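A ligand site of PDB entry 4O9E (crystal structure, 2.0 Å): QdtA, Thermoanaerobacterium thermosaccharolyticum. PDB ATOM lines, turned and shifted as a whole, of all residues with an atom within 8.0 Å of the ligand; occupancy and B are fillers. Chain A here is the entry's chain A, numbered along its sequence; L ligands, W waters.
NZ of Lys 72 is in hydrogen-bond range of O2 of the ligand.
The side-chain carboxylate (OE2) of Glu 98 is in hydrogen-bond range of a nitrogen (N2) of the ligand (3.3 Å).
NH1 of Arg 70 is in salt-bridge range of OE1 of Glu 98.
O of Lys 72 sits at hydrogen-bond distance from N of Trp 96, at 2.9 Å.
OE2 of Glu 98 is in hydrogen-bond range of NE1 of Trp 96, 2.8 Å away.
The nearest printed residue that does not touch the ligand is Tyr 125 (4.1 Å).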
ATOM      1  N   TYR A  50      32.408 -21.798   7.961  1.00  0.00           N
ATOM      2  CA  TYR A  50      31.487 -22.773   8.551  1.00  0.00           C
ATOM      3  C   TYR A  50      31.487 -22.657  10.070  1.00  0.00           C
ATOM      4  O   TYR A  50      31.752 -23.603  10.822  1.00  0.00           O
ATOM      5  CB  TYR A  50      31.844 -24.203   8.148  1.00  0.00           C
ATOM      6  CG  TYR A  50      31.877 -24.453   6.653  1.00  0.00           C
ATOM      7  CD1 TYR A  50      30.702 -24.587   5.920  1.00  0.00           C
ATOM      8  CD2 TYR A  50      33.088 -24.598   5.982  1.00  0.00           C
ATOM      9  CE1 TYR A  50      30.720 -24.833   4.559  1.00  0.00           C
ATOM     10  CE2 TYR A  50      33.133 -24.866   4.626  1.00  0.00           C
ATOM     11  CZ  TYR A  50      31.939 -24.979   3.929  1.00  0.00           C
ATOM     12  OH  TYR A  50      31.945 -25.239   2.581  1.00  0.00           O
ATOM     13  N   HIS A  51      31.190 -21.461  10.524  1.00  0.00           N
ATOM     14  CA  HIS A  51      31.042 -21.263  11.958  1.00  0.00           C
ATOM     15  C   HIS A  51      30.441 -19.904  12.202  1.00  0.00           C
ATOM     16  O   HIS A  51      30.288 -19.083  11.298  1.00  0.00           O
ATOM     17  CB  HIS A  51      32.380 -21.364  12.671  1.00  0.00           C
ATOM     18  CG  HIS A  51      33.468 -20.516  12.074  1.00  0.00           C
ATOM     19  ND1 HIS A  51      33.469 -19.150  12.168  1.00  0.00           N
ATOM     20  CD2 HIS A  51      34.620 -20.867  11.464  1.00  0.00           C
ATOM     21  CE1 HIS A  51      34.579 -18.674  11.635  1.00  0.00           C
ATOM     22  NE2 HIS A  51      35.290 -19.696  11.182  1.00  0.00           N
ATOM     23  N   ARG A  70      29.561 -15.670   2.466  1.00  0.00           N
ATOM     24  CA  ARG A  70      28.184 -16.161   2.597  1.00  0.00           C
ATOM     25  C   ARG A  70      27.839 -16.071   4.077  1.00  0.00           C
ATOM     26  O   ARG A  70      28.445 -16.763   4.901  1.00  0.00           O
ATOM     27  CB  ARG A  70      28.044 -17.623   2.175  1.00  0.00           C
ATOM     28  CG  ARG A  70      26.677 -18.237   2.440  1.00  0.00           C
ATOM     29  CD  ARG A  70      26.536 -19.660   1.885  1.00  0.00           C
ATOM     30  NE  ARG A  70      26.967 -19.678   0.490  1.00  0.00           N
ATOM     31  CZ  ARG A  70      28.077 -20.247   0.019  1.00  0.00           C
ATOM     32  NH1 ARG A  70      28.896 -20.946   0.806  1.00  0.00           N
ATOM     33  NH2 ARG A  70      28.342 -20.102  -1.275  1.00  0.00           N
ATOM     34  N   LYS A  72      24.664 -16.136   6.938  1.00  0.00           N
ATOM     35  CA  LYS A  72      23.375 -16.782   7.161  1.00  0.00           C
ATOM     36  C   LYS A  72      22.977 -16.573   8.589  1.00  0.00           C
ATOM     37  O   LYS A  72      23.806 -16.736   9.487  1.00  0.00           O
ATOM     38  CB  LYS A  72      23.542 -18.284   6.990  1.00  0.00           C
ATOM     39  CG  LYS A  72      23.963 -18.705   5.595  1.00  0.00           C
ATOM     40  CD  LYS A  72      24.251 -20.195   5.454  1.00  0.00           C
ATOM     41  CE  LYS A  72      23.145 -21.018   6.096  1.00  0.00           C
ATOM     42  NZ  LYS A  72      22.995 -22.216   5.235  1.00  0.00           N
ATOM     43  N   GLU A  77      19.790 -15.308   3.965  1.00  0.00           N
ATOM     44  CA  GLU A  77      21.146 -15.590   3.526  1.00  0.00           C
ATOM     45  C   GLU A  77      21.540 -14.519   2.544  1.00  0.00           C
ATOM     46  O   GLU A  77      20.674 -14.029   1.809  1.00  0.00           O
ATOM     47  CB  GLU A  77      21.314 -17.027   3.039  1.00  0.00           C
ATOM     48  CG  GLU A  77      22.099 -17.158   1.750  1.00  0.00           C
ATOM     49  CD  GLU A  77      22.584 -18.564   1.466  1.00  0.00           C
ATOM     50  OE1 GLU A  77      23.238 -18.701   0.414  1.00  0.00           O
ATOM     51  OE2 GLU A  77      22.335 -19.512   2.232  1.00  0.00           O
ATOM     52  N   TRP A  96      26.275 -16.910  10.912  1.00  0.00           N
ATOM     53  CA  TRP A  96      27.036 -18.033  10.414  1.00  0.00           C
ATOM     54  C   TRP A  96      27.790 -17.574   9.179  1.00  0.00           C
ATOM     55  O   TRP A  96      27.291 -16.840   8.325  1.00  0.00           O
ATOM     56  CB  TRP A  96      26.122 -19.241  10.176  1.00  0.00           C
ATOM     57  CG  TRP A  96      26.785 -20.467   9.548  1.00  0.00           C
ATOM     58  CD1 TRP A  96      27.029 -20.674   8.210  1.00  0.00           C
ATOM     59  CD2 TRP A  96      27.334 -21.596  10.226  1.00  0.00           C
ATOM     60  NE1 TRP A  96      27.710 -21.853   8.024  1.00  0.00           N
ATOM     61  CE2 TRP A  96      27.834 -22.478   9.229  1.00  0.00           C
ATOM     62  CE3 TRP A  96      27.379 -22.001  11.558  1.00  0.00           C
ATOM     63  CZ2 TRP A  96      28.450 -23.679   9.533  1.00  0.00           C
ATOM     64  CZ3 TRP A  96      27.943 -23.218  11.856  1.00  0.00           C
ATOM     65  CH2 TRP A  96      28.469 -24.054  10.848  1.00  0.00           C
ATOM     66  N   ARG A  97      29.068 -17.892   9.048  1.00  0.00           N
ATOM     67  CA  ARG A  97      29.644 -17.501   7.778  1.00  0.00           C
ATOM     68  C   ARG A  97      30.496 -18.536   7.062  1.00  0.00           C
ATOM     69  O   ARG A  97      31.111 -19.384   7.689  1.00  0.00           O
ATOM     70  CB  ARG A  97      30.459 -16.232   7.916  1.00  0.00           C
ATOM     71  CG  ARG A  97      31.716 -16.372   8.762  1.00  0.00           C
ATOM     72  CD  ARG A  97      32.573 -15.156   8.470  1.00  0.00           C
ATOM     73  NE  ARG A  97      33.933 -15.321   8.982  1.00  0.00           N
ATOM     74  CZ  ARG A  97      34.228 -15.263  10.261  1.00  0.00           C
ATOM     75  NH1 ARG A  97      33.233 -15.017  11.116  1.00  0.00           N
ATOM     76  NH2 ARG A  97      35.495 -15.410  10.633  1.00  0.00           N
ATOM     77  N   GLU A  98      30.629 -18.316   5.748  1.00  0.00           N
ATOM     78  CA  GLU A  98      31.459 -19.160   4.910  1.00  0.00           C
ATOM     79  C   GLU A  98      32.092 -18.209   3.910  1.00  0.00           C
ATOM     80  O   GLU A  98      31.538 -17.167   3.585  1.00  0.00           O
ATOM     81  CB  GLU A  98      30.663 -20.291   4.262  1.00  0.00           C
ATOM     82  CG  GLU A  98      29.905 -21.205   5.220  1.00  0.00           C
ATOM     83  CD  GLU A  98      28.732 -21.948   4.592  1.00  0.00           C
ATOM     84  OE1 GLU A  98      28.623 -21.874   3.353  1.00  0.00           O
ATOM     85  OE2 GLU A  98      27.908 -22.580   5.312  1.00  0.00           O
ATOM     86  N   ARG A 123      30.859 -24.339  15.677  1.00  0.00           N
ATOM     87  CA  ARG A 123      31.244 -25.008  14.438  1.00  0.00           C
ATOM     88  C   ARG A 123      30.233 -26.085  14.011  1.00  0.00           C
ATOM     89  O   ARG A 123      30.261 -26.582  12.889  1.00  0.00           O
ATOM     90  CB  ARG A 123      32.608 -25.658  14.641  1.00  0.00           C
ATOM     91  CG  ARG A 123      33.741 -24.684  14.972  1.00  0.00           C
ATOM     92  CD  ARG A 123      35.050 -25.438  14.984  1.00  0.00           C
ATOM     93  NE  ARG A 123      36.228 -24.590  15.090  1.00  0.00           N
ATOM     94  CZ  ARG A 123      36.801 -23.871  14.128  1.00  0.00           C
ATOM     95  NH1 ARG A 123      36.282 -23.759  12.906  1.00  0.00           N
ATOM     96  NH2 ARG A 123      37.919 -23.208  14.415  1.00  0.00           N
ATOM     97  N   ASN A 124      29.341 -26.462  14.923  1.00  0.00           N
ATOM     98  CA  ASN A 124      28.283 -27.440  14.697  1.00  0.00           C
ATOM     99  C   ASN A 124      27.066 -26.691  14.181  1.00  0.00           C
ATOM    100  O   ASN A 124      26.439 -25.889  14.877  1.00  0.00           O
ATOM    101  CB  ASN A 124      27.956 -28.181  15.988  1.00  0.00           C
ATOM    102  CG  ASN A 124      26.768 -29.121  15.843  1.00  0.00           C
ATOM    103  OD1 ASN A 124      25.582 -28.763  15.852  1.00  0.00           O
ATOM    104  ND2 ASN A 124      27.093 -30.383  15.716  1.00  0.00           N
ATOM    105  N   TYR A 125      26.751 -26.913  12.903  1.00  0.00           N
ATOM    106  CA  TYR A 125      25.655 -26.186  12.322  1.00  0.00           C
ATOM    107  C   TYR A 125      24.331 -26.364  13.055  1.00  0.00           C
ATOM    108  O   TYR A 125      23.565 -25.415  13.154  1.00  0.00           O
ATOM    109  CB  TYR A 125      25.536 -26.518  10.836  1.00  0.00           C
ATOM    110  CG  TYR A 125      24.454 -25.715  10.154  1.00  0.00           C
ATOM    111  CD1 TYR A 125      24.661 -24.405   9.769  1.00  0.00           C
ATOM    112  CD2 TYR A 125      23.216 -26.287   9.873  1.00  0.00           C
ATOM    113  CE1 TYR A 125      23.668 -23.671   9.146  1.00  0.00           C
ATOM    114  CE2 TYR A 125      22.231 -25.585   9.217  1.00  0.00           C
ATOM    115  CZ  TYR A 125      22.478 -24.292   8.786  1.00  0.00           C
ATOM    116  OH  TYR A 125      21.493 -23.589   8.130  1.00  0.00           O
ATOM    117  N   ASP A 126      24.032 -27.550  13.593  1.00  0.00           N
ATOM    118  CA  ASP A 126      22.749 -27.734  14.286  1.00  0.00           C
ATOM    119  C   ASP A 126      22.676 -26.959  15.614  1.00  0.00           C
ATOM    120  O   ASP A 126      21.644 -26.433  16.035  1.00  0.00           O
ATOM    121  CB  ASP A 126      22.467 -29.218  14.518  1.00  0.00           C
ATOM    122  CG  ASP A 126      22.215 -30.000  13.239  1.00  0.00           C
ATOM    123  OD1 ASP A 126      21.755 -29.504  12.209  1.00  0.00           O
ATOM    124  OD2 ASP A 126      22.540 -31.203  13.262  1.00  0.00           O
ATOM    125  N   ILE A 129      22.017 -23.230  14.589  1.00  0.00           N
ATOM    126  CA  ILE A 129      20.627 -22.900  14.303  1.00  0.00           C
ATOM    127  C   ILE A 129      19.822 -22.935  15.583  1.00  0.00           C
ATOM    128  O   ILE A 129      18.970 -22.085  15.778  1.00  0.00           O
ATOM    129  CB  ILE A 129      20.024 -23.843  13.226  1.00  0.00           C
ATOM    130  CG1 ILE A 129      20.642 -23.558  11.849  1.00  0.00           C
ATOM    131  CG2 ILE A 129      18.502 -23.840  13.218  1.00  0.00           C
ATOM    132  CD1 ILE A 129      20.231 -22.307  11.111  1.00  0.00           C
HETATM  133  N1  LIG L   1      24.971 -27.242   6.184  1.00  0.00           N
HETATM  134  C1  LIG L   1      26.066 -26.489   6.324  1.00  0.00           C
HETATM  135  O1  LIG L   1      27.085 -26.950   6.887  1.00  0.00           O
HETATM  136  N2  LIG L   1      26.068 -25.237   5.848  1.00  0.00           N
HETATM  137  C2  LIG L   1      24.997 -24.731   5.231  1.00  0.00           C
HETATM  138  O2  LIG L   1      25.138 -23.552   4.828  1.00  0.00           O
HETATM  139  C3  LIG L   1      23.764 -25.544   5.074  1.00  0.00           C
HETATM  140  C4  LIG L   1      22.443 -25.200   4.424  1.00  0.00           C
HETATM  141  C5  LIG L   1      23.847 -26.825   5.600  1.00  0.00           C
HETATM  142  O   HOH W   1      29.732 -27.712   7.402  1.00  0.00           O
